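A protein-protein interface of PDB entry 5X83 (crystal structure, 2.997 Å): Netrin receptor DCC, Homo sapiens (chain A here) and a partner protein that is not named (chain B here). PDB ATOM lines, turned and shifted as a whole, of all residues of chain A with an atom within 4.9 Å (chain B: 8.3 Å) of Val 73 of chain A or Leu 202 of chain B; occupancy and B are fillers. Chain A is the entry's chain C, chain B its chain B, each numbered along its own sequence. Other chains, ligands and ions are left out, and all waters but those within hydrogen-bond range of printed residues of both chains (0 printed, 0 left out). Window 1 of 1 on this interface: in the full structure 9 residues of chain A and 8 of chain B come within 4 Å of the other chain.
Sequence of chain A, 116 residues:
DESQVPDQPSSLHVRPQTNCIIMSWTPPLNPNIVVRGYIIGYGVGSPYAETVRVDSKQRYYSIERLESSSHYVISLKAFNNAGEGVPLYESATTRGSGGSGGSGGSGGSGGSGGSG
O of Gly 43 of chain A sits at hydrogen-bond distance from N of Val 73 of chain A, at 2.9 Å.
The backbone carbonyl oxygen of Ile 74 of chain A lies within hydrogen-bond range of the backbone NH of Glu 90 of chain A (2.9 Å).
Of the 13 printed residues of chain B, 7 touch a printed residue of chain A.
Hydrophobic or aromatic side chains of chain B within 4 Å of the printed part of chain A: Pro 118, Leu 172, Leu 202 and Phe 206.
Along chain B the printed residues that touch a printed residue of chain A span positions 116 to 206.
Among the printed residues, no Asp or Glu carboxylate lies within 4 Å of a Lys or Arg side-chain nitrogen of the other chain.
The side-chain hydroxyl (OG) of Ser 91 of chain A lies within hydrogen-bond range of the guanidinium group (NH2) of Arg 119 of chain B.
Gly 43 of chain A touches none of the printed residues of chain B.
Of the printed residues of chain B, Pro 47 of chain A touches Phe 206.
Of the printed residues of chain B, Val 73 of chain A touches Leu 202 (3.8 Å).
Of chain A, only Val 73, Tyr 89, Glu 90 and Ser 91 come within 4 Å of Leu 202 of chain B.
Of the printed residues of chain A, Glu 203 of chain B touches Tyr 89 (3.8 Å).
Among the printed residues, merely in contact across the chains: Gly 45 of chain A with Gly 116 of chain B (3.6 Å), Gly 45 of chain A with Pro 118 of chain B (3.4 Å), Gly 45 of chain A with Phe 206 of chain B (3.6 Å), Ser 46 of chain A with Phe 206 of chain B (3.9 Å), Pro 47 of chain A with Phe 206 of chain B (3.5 Å), His 71 of chain A with Arg 119 of chain B (3.4 Å), Val 73 of chain A with Leu 202 of chain B (3.8 Å), Tyr 89 of chain A with Leu 202 of chain B (3.5 Å), Tyr 89 of chain A with Glu 203 of chain B (3.8 Å), Tyr 89 of chain A with Phe 206 of chain B (3.7 Å), Glu 90 of chain A with Leu 202 of chain B (3.8 Å), Ser 91 of chain A with Leu 172 of chain B (3.5 Å) and Ser 91 of chain A with Leu 202 of chain B (3.7 Å).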
ATOM      1  N   GLY A  41      -4.830 -12.899  -0.199  1.00  0.00           N
ATOM      2  CA  GLY A  41      -5.459 -14.009   0.487  1.00  0.00           C
ATOM      3  C   GLY A  41      -5.261 -15.307  -0.267  1.00  0.00           C
ATOM      4  O   GLY A  41      -5.257 -15.314  -1.499  1.00  0.00           O
ATOM      5  N   TYR A  42      -5.094 -16.405   0.467  1.00  0.00           N
ATOM      6  CA  TYR A  42      -4.933 -17.712  -0.163  1.00  0.00           C
ATOM      7  C   TYR A  42      -5.390 -18.868   0.726  1.00  0.00           C
ATOM      8  O   TYR A  42      -5.475 -18.737   1.947  1.00  0.00           O
ATOM      9  CB  TYR A  42      -3.477 -17.934  -0.576  1.00  0.00           C
ATOM     10  CG  TYR A  42      -2.488 -17.980   0.568  1.00  0.00           C
ATOM     11  CD1 TYR A  42      -1.940 -16.815   1.091  1.00  0.00           C
ATOM     12  CD2 TYR A  42      -2.087 -19.194   1.112  1.00  0.00           C
ATOM     13  CE1 TYR A  42      -1.028 -16.860   2.130  1.00  0.00           C
ATOM     14  CE2 TYR A  42      -1.179 -19.249   2.148  1.00  0.00           C
ATOM     15  CZ  TYR A  42      -0.652 -18.082   2.653  1.00  0.00           C
ATOM     16  OH  TYR A  42       0.252 -18.142   3.686  1.00  0.00           O
ATOM     17  N   GLY A  43      -5.685 -19.998   0.091  1.00  0.00           N
ATOM     18  CA  GLY A  43      -6.121 -21.196   0.784  1.00  0.00           C
ATOM     19  C   GLY A  43      -6.440 -22.283  -0.226  1.00  0.00           C
ATOM     20  O   GLY A  43      -6.224 -22.103  -1.423  1.00  0.00           O
ATOM     21  N   GLY A  45      -9.370 -24.040  -2.088  1.00  0.00           N
ATOM     22  CA  GLY A  45     -10.777 -23.868  -2.405  1.00  0.00           C
ATOM     23  C   GLY A  45     -11.426 -22.651  -1.770  1.00  0.00           C
ATOM     24  O   GLY A  45     -12.652 -22.522  -1.765  1.00  0.00           O
ATOM     25  N   SER A  46     -10.597 -21.759  -1.235  1.00  0.00           N
ATOM     26  CA  SER A  46     -11.069 -20.561  -0.548  1.00  0.00           C
ATOM     27  C   SER A  46      -9.919 -19.585  -0.330  1.00  0.00           C
ATOM     28  O   SER A  46      -8.837 -19.987   0.085  1.00  0.00           O
ATOM     29  CB  SER A  46     -11.710 -20.926   0.793  1.00  0.00           C
ATOM     30  OG  SER A  46     -12.360 -19.807   1.367  1.00  0.00           O
ATOM     31  N   PRO A  47     -10.147 -18.296  -0.612  1.00  0.00           N
ATOM     32  CA  PRO A  47      -9.113 -17.279  -0.419  1.00  0.00           C
ATOM     33  C   PRO A  47      -9.197 -16.597   0.944  1.00  0.00           C
ATOM     34  O   PRO A  47      -8.552 -15.569   1.149  1.00  0.00           O
ATOM     35  CB  PRO A  47      -9.402 -16.282  -1.540  1.00  0.00           C
ATOM     36  CG  PRO A  47     -10.889 -16.439  -1.824  1.00  0.00           C
ATOM     37  CD  PRO A  47     -11.378 -17.712  -1.168  1.00  0.00           C
ATOM     38  N   HIS A  71      -4.775 -27.586  -5.278  1.00  0.00           N
ATOM     39  CA  HIS A  71      -5.462 -26.497  -5.956  1.00  0.00           C
ATOM     40  C   HIS A  71      -5.693 -25.313  -5.023  1.00  0.00           C
ATOM     41  O   HIS A  71      -6.617 -25.322  -4.212  1.00  0.00           O
ATOM     42  CB  HIS A  71      -6.790 -26.989  -6.530  1.00  0.00           C
ATOM     43  CG  HIS A  71      -6.631 -27.984  -7.638  1.00  0.00           C
ATOM     44  ND1 HIS A  71      -5.976 -27.688  -8.813  1.00  0.00           N
ATOM     45  CD2 HIS A  71      -7.041 -29.269  -7.748  1.00  0.00           C
ATOM     46  CE1 HIS A  71      -5.988 -28.749  -9.601  1.00  0.00           C
ATOM     47  NE2 HIS A  71      -6.629 -29.721  -8.979  1.00  0.00           N
ATOM     48  N   TYR A  72      -4.850 -24.294  -5.150  1.00  0.00           N
ATOM     49  CA  TYR A  72      -4.939 -23.118  -4.294  1.00  0.00           C
ATOM     50  C   TYR A  72      -5.712 -21.996  -4.977  1.00  0.00           C
ATOM     51  O   TYR A  72      -5.723 -21.892  -6.204  1.00  0.00           O
ATOM     52  CB  TYR A  72      -3.541 -22.636  -3.901  1.00  0.00           C
ATOM     53  CG  TYR A  72      -2.870 -23.515  -2.869  1.00  0.00           C
ATOM     54  CD1 TYR A  72      -3.091 -23.320  -1.512  1.00  0.00           C
ATOM     55  CD2 TYR A  72      -2.020 -24.542  -3.254  1.00  0.00           C
ATOM     56  CE1 TYR A  72      -2.481 -24.124  -0.568  1.00  0.00           C
ATOM     57  CE2 TYR A  72      -1.406 -25.350  -2.319  1.00  0.00           C
ATOM     58  CZ  TYR A  72      -1.639 -25.138  -0.979  1.00  0.00           C
ATOM     59  OH  TYR A  72      -1.026 -25.945  -0.048  1.00  0.00           O
ATOM     60  N   VAL A  73      -6.373 -21.169  -4.173  1.00  0.00           N
ATOM     61  CA  VAL A  73      -7.106 -20.020  -4.690  1.00  0.00           C
ATOM     62  C   VAL A  73      -6.527 -18.735  -4.112  1.00  0.00           C
ATOM     63  O   VAL A  73      -6.407 -18.591  -2.896  1.00  0.00           O
ATOM     64  CB  VAL A  73      -8.606 -20.105  -4.365  1.00  0.00           C
ATOM     65  CG1 VAL A  73      -9.325 -18.864  -4.863  1.00  0.00           C
ATOM     66  CG2 VAL A  73      -9.210 -21.350  -4.987  1.00  0.00           C
ATOM     67  N   ILE A  74      -6.163 -17.805  -4.988  1.00  0.00           N
ATOM     68  CA  ILE A  74      -5.491 -16.581  -4.571  1.00  0.00           C
ATOM     69  C   ILE A  74      -6.310 -15.336  -4.895  1.00  0.00           C
ATOM     70  O   ILE A  74      -6.779 -15.161  -6.019  1.00  0.00           O
ATOM     71  CB  ILE A  74      -4.108 -16.452  -5.235  1.00  0.00           C
ATOM     72  CG1 ILE A  74      -3.315 -17.749  -5.080  1.00  0.00           C
ATOM     73  CG2 ILE A  74      -3.342 -15.287  -4.641  1.00  0.00           C
ATOM     74  CD1 ILE A  74      -1.986 -17.737  -5.797  1.00  0.00           C
ATOM     75  N   SER A  75      -6.481 -14.476  -3.897  1.00  0.00           N
ATOM     76  CA  SER A  75      -7.184 -13.216  -4.086  1.00  0.00           C
ATOM     77  C   SER A  75      -6.229 -12.040  -3.948  1.00  0.00           C
ATOM     78  O   SER A  75      -5.184 -12.148  -3.307  1.00  0.00           O
ATOM     79  CB  SER A  75      -8.325 -13.078  -3.078  1.00  0.00           C
ATOM     80  OG  SER A  75      -7.826 -12.736  -1.797  1.00  0.00           O
ATOM     81  N   TYR A  89      -9.310 -12.483  -8.666  1.00  0.00           N
ATOM     82  CA  TYR A  89      -9.165 -13.873  -8.261  1.00  0.00           C
ATOM     83  C   TYR A  89      -8.343 -14.653  -9.275  1.00  0.00           C
ATOM     84  O   TYR A  89      -8.426 -14.397 -10.476  1.00  0.00           O
ATOM     85  CB  TYR A  89     -10.535 -14.525  -8.086  1.00  0.00           C
ATOM     86  CG  TYR A  89     -11.386 -13.916  -6.994  1.00  0.00           C
ATOM     87  CD1 TYR A  89     -11.273 -14.346  -5.680  1.00  0.00           C
ATOM     88  CD2 TYR A  89     -12.309 -12.918  -7.279  1.00  0.00           C
ATOM     89  CE1 TYR A  89     -12.052 -13.798  -4.679  1.00  0.00           C
ATOM     90  CE2 TYR A  89     -13.093 -12.363  -6.287  1.00  0.00           C
ATOM     91  CZ  TYR A  89     -12.960 -12.806  -4.988  1.00  0.00           C
ATOM     92  OH  TYR A  89     -13.735 -12.256  -3.992  1.00  0.00           O
ATOM     93  N   GLU A  90      -7.558 -15.608  -8.787  1.00  0.00           N
ATOM     94  CA  GLU A  90      -6.719 -16.435  -9.650  1.00  0.00           C
ATOM     95  C   GLU A  90      -6.527 -17.837  -9.090  1.00  0.00           C
ATOM     96  O   GLU A  90      -6.196 -18.011  -7.918  1.00  0.00           O
ATOM     97  CB  GLU A  90      -5.351 -15.780  -9.870  1.00  0.00           C
ATOM     98  CG  GLU A  90      -5.323 -14.735 -10.973  1.00  0.00           C
ATOM     99  CD  GLU A  90      -5.520 -15.338 -12.352  1.00  0.00           C
ATOM    100  OE1 GLU A  90      -5.272 -16.552 -12.515  1.00  0.00           O
ATOM    101  OE2 GLU A  90      -5.928 -14.599 -13.274  1.00  0.00           O
ATOM    102  N   SER A  91      -6.726 -18.833  -9.945  1.00  0.00           N
ATOM    103  CA  SER A  91      -6.517 -20.221  -9.568  1.00  0.00           C
ATOM    104  C   SER A  91      -5.095 -20.658  -9.911  1.00  0.00           C
ATOM    105  O   SER A  91      -4.607 -20.400 -11.012  1.00  0.00           O
ATOM    106  CB  SER A  91      -7.536 -21.121 -10.266  1.00  0.00           C
ATOM    107  OG  SER A  91      -7.504 -22.431  -9.731  1.00  0.00           O
ATOM    108  N   GLY B 116     -17.014 -27.077   1.237  1.00  0.00           N
ATOM    109  CA  GLY B 116     -16.692 -25.867   0.501  1.00  0.00           C
ATOM    110  C   GLY B 116     -15.435 -26.029  -0.326  1.00  0.00           C
ATOM    111  O   GLY B 116     -14.559 -25.163  -0.326  1.00  0.00           O
ATOM    112  N   PRO B 118     -14.382 -26.379  -4.041  1.00  0.00           N
ATOM    113  CA  PRO B 118     -14.683 -26.315  -5.475  1.00  0.00           C
ATOM    114  C   PRO B 118     -13.776 -27.231  -6.290  1.00  0.00           C
ATOM    115  O   PRO B 118     -12.990 -27.982  -5.709  1.00  0.00           O
ATOM    116  CB  PRO B 118     -14.445 -24.841  -5.823  1.00  0.00           C
ATOM    117  CG  PRO B 118     -13.518 -24.344  -4.774  1.00  0.00           C
ATOM    118  CD  PRO B 118     -13.865 -25.102  -3.526  1.00  0.00           C
ATOM    119  N   ARG B 119     -13.910 -27.176  -7.615  1.00  0.00           N
ATOM    120  CA  ARG B 119     -13.171 -28.051  -8.529  1.00  0.00           C
ATOM    121  C   ARG B 119     -13.560 -29.520  -8.357  1.00  0.00           C
ATOM    122  O   ARG B 119     -12.968 -30.404  -8.978  1.00  0.00           O
ATOM    123  CB  ARG B 119     -11.656 -27.891  -8.352  1.00  0.00           C
ATOM    124  CG  ARG B 119     -11.010 -26.895  -9.300  1.00  0.00           C
ATOM    125  CD  ARG B 119      -9.500 -27.077  -9.310  1.00  0.00           C
ATOM    126  NE  ARG B 119      -8.865 -26.403 -10.439  1.00  0.00           N
ATOM    127  CZ  ARG B 119      -8.186 -25.267 -10.348  1.00  0.00           C
ATOM    128  NH1 ARG B 119      -8.045 -24.669  -9.173  1.00  0.00           N
ATOM    129  NH2 ARG B 119      -7.642 -24.728 -11.432  1.00  0.00           N
ATOM    130  N   LEU B 172     -12.110 -24.609 -13.582  1.00  0.00           N
ATOM    131  CA  LEU B 172     -12.989 -23.547 -13.111  1.00  0.00           C
ATOM    132  C   LEU B 172     -13.545 -22.749 -14.284  1.00  0.00           C
ATOM    133  O   LEU B 172     -12.828 -22.464 -15.245  1.00  0.00           O
ATOM    134  CB  LEU B 172     -12.242 -22.631 -12.146  1.00  0.00           C
ATOM    135  CG  LEU B 172     -11.895 -23.287 -10.810  1.00  0.00           C
ATOM    136  CD1 LEU B 172     -10.999 -22.380  -9.980  1.00  0.00           C
ATOM    137  CD2 LEU B 172     -13.161 -23.655 -10.048  1.00  0.00           C
ATOM    138  N   ASP B 173     -14.823 -22.396 -14.191  1.00  0.00           N
ATOM    139  CA  ASP B 173     -15.548 -21.735 -15.276  1.00  0.00           C
ATOM    140  C   ASP B 173     -15.389 -22.490 -16.593  1.00  0.00           C
ATOM    141  O   ASP B 173     -14.775 -21.995 -17.537  1.00  0.00           O
ATOM    142  CB  ASP B 173     -15.078 -20.288 -15.439  1.00  0.00           C
ATOM    143  CG  ASP B 173     -15.962 -19.490 -16.381  1.00  0.00           C
ATOM    144  OD1 ASP B 173     -17.094 -19.940 -16.658  1.00  0.00           O
ATOM    145  OD2 ASP B 173     -15.520 -18.417 -16.846  1.00  0.00           O
ATOM    146  N   THR B 199     -19.404 -25.244 -13.985  1.00  0.00           N
ATOM    147  CA  THR B 199     -18.660 -24.905 -12.783  1.00  0.00           C
ATOM    148  C   THR B 199     -18.599 -23.387 -12.643  1.00  0.00           C
ATOM    149  O   THR B 199     -18.508 -22.668 -13.639  1.00  0.00           O
ATOM    150  CB  THR B 199     -17.238 -25.491 -12.814  1.00  0.00           C
ATOM    151  OG1 THR B 199     -16.550 -25.017 -13.977  1.00  0.00           O
ATOM    152  CG2 THR B 199     -17.295 -27.008 -12.862  1.00  0.00           C
ATOM    153  N   LEU B 200     -18.648 -22.901 -11.408  1.00  0.00           N
ATOM    154  CA  LEU B 200     -18.688 -21.464 -11.166  1.00  0.00           C
ATOM    155  C   LEU B 200     -17.295 -20.854 -11.248  1.00  0.00           C
ATOM    156  O   LEU B 200     -16.292 -21.564 -11.178  1.00  0.00           O
ATOM    157  CB  LEU B 200     -19.311 -21.167  -9.802  1.00  0.00           C
ATOM    158  CG  LEU B 200     -20.825 -21.362  -9.697  1.00  0.00           C
ATOM    159  CD1 LEU B 200     -21.299 -21.175  -8.263  1.00  0.00           C
ATOM    160  CD2 LEU B 200     -21.547 -20.405 -10.635  1.00  0.00           C
ATOM    161  N   LYS B 201     -17.237 -19.537 -11.415  1.00  0.00           N
ATOM    162  CA  LYS B 201     -15.964 -18.829 -11.399  1.00  0.00           C
ATOM    163  C   LYS B 201     -15.726 -18.230 -10.017  1.00  0.00           C
ATOM    164  O   LYS B 201     -16.673 -17.975  -9.272  1.00  0.00           O
ATOM    165  CB  LYS B 201     -15.933 -17.740 -12.474  1.00  0.00           C
ATOM    166  CG  LYS B 201     -14.547 -17.157 -12.732  1.00  0.00           C
ATOM    167  CD  LYS B 201     -13.506 -18.263 -12.870  1.00  0.00           C
ATOM    168  CE  LYS B 201     -12.231 -17.764 -13.535  1.00  0.00           C
ATOM    169  NZ  LYS B 201     -11.192 -18.831 -13.618  1.00  0.00           N
ATOM    170  N   LEU B 202     -14.459 -18.012  -9.683  1.00  0.00           N
ATOM    171  CA  LEU B 202     -14.069 -17.544  -8.359  1.00  0.00           C
ATOM    172  C   LEU B 202     -14.717 -16.209  -8.002  1.00  0.00           C
ATOM    173  O   LEU B 202     -15.003 -15.943  -6.834  1.00  0.00           O
ATOM    174  CB  LEU B 202     -12.548 -17.422  -8.279  1.00  0.00           C
ATOM    175  CG  LEU B 202     -11.747 -18.625  -8.778  1.00  0.00           C
ATOM    176  CD1 LEU B 202     -10.344 -18.207  -9.191  1.00  0.00           C
ATOM    177  CD2 LEU B 202     -11.691 -19.695  -7.696  1.00  0.00           C
ATOM    178  N   GLU B 203     -14.948 -15.377  -9.014  1.00  0.00           N
ATOM    179  CA  GLU B 203     -15.588 -14.081  -8.819  1.00  0.00           C
ATOM    180  C   GLU B 203     -16.988 -14.203  -8.222  1.00  0.00           C
ATOM    181  O   GLU B 203     -17.321 -13.524  -7.250  1.00  0.00           O
ATOM    182  CB  GLU B 203     -15.658 -13.320 -10.144  1.00  0.00           C
ATOM    183  CG  GLU B 203     -16.536 -12.078 -10.101  1.00  0.00           C
ATOM    184  CD  GLU B 203     -16.416 -11.234 -11.356  1.00  0.00           C
ATOM    185  OE1 GLU B 203     -16.215 -11.811 -12.445  1.00  0.00           O
ATOM    186  OE2 GLU B 203     -16.522  -9.992 -11.252  1.00  0.00           O
ATOM    187  N   VAL B 204     -17.803 -15.073  -8.810  1.00  0.00           N
ATOM    188  CA  VAL B 204     -19.189 -15.242  -8.383  1.00  0.00           C
ATOM    189  C   VAL B 204     -19.307 -16.011  -7.066  1.00  0.00           C
ATOM    190  O   VAL B 204     -20.175 -15.717  -6.242  1.00  0.00           O
ATOM    191  CB  VAL B 204     -20.013 -15.970  -9.469  1.00  0.00           C
ATOM    192  CG1 VAL B 204     -21.472 -16.091  -9.052  1.00  0.00           C
ATOM    193  CG2 VAL B 204     -19.900 -15.237 -10.797  1.00  0.00           C
ATOM    194  N   LEU B 205     -18.420 -16.979  -6.864  1.00  0.00           N
ATOM    195  CA  LEU B 205     -18.512 -17.875  -5.714  1.00  0.00           C
ATOM    196  C   LEU B 205     -18.189 -17.176  -4.394  1.00  0.00           C
ATOM    197  O   LEU B 205     -18.644 -17.601  -3.330  1.00  0.00           O
ATOM    198  CB  LEU B 205     -17.586 -19.078  -5.910  1.00  0.00           C
ATOM    199  CG  LEU B 205     -17.758 -20.242  -4.932  1.00  0.00           C
ATOM    200  CD1 LEU B 205     -19.216 -20.667  -4.860  1.00  0.00           C
ATOM    201  CD2 LEU B 205     -16.878 -21.414  -5.338  1.00  0.00           C
ATOM    202  N   PHE B 206     -17.404 -16.104  -4.460  1.00  0.00           N
ATOM    203  CA  PHE B 206     -17.017 -15.376  -3.256  1.00  0.00           C
ATOM    204  C   PHE B 206     -17.498 -13.927  -3.300  1.00  0.00           C
ATOM    205  O   PHE B 206     -18.490 -13.573  -2.661  1.00  0.00           O
ATOM    206  CB  PHE B 206     -15.498 -15.426  -3.069  1.00  0.00           C
ATOM    207  CG  PHE B 206     -14.944 -16.822  -3.023  1.00  0.00           C
ATOM    208  CD1 PHE B 206     -15.162 -17.637  -1.924  1.00  0.00           C
ATOM    209  CD2 PHE B 206     -14.206 -17.324  -4.082  1.00  0.00           C
ATOM    210  CE1 PHE B 206     -14.655 -18.922  -1.882  1.00  0.00           C
ATOM    211  CE2 PHE B 206     -13.696 -18.608  -4.046  1.00  0.00           C
ATOM    212  CZ  PHE B 206     -13.920 -19.407  -2.945  1.00  0.00           C
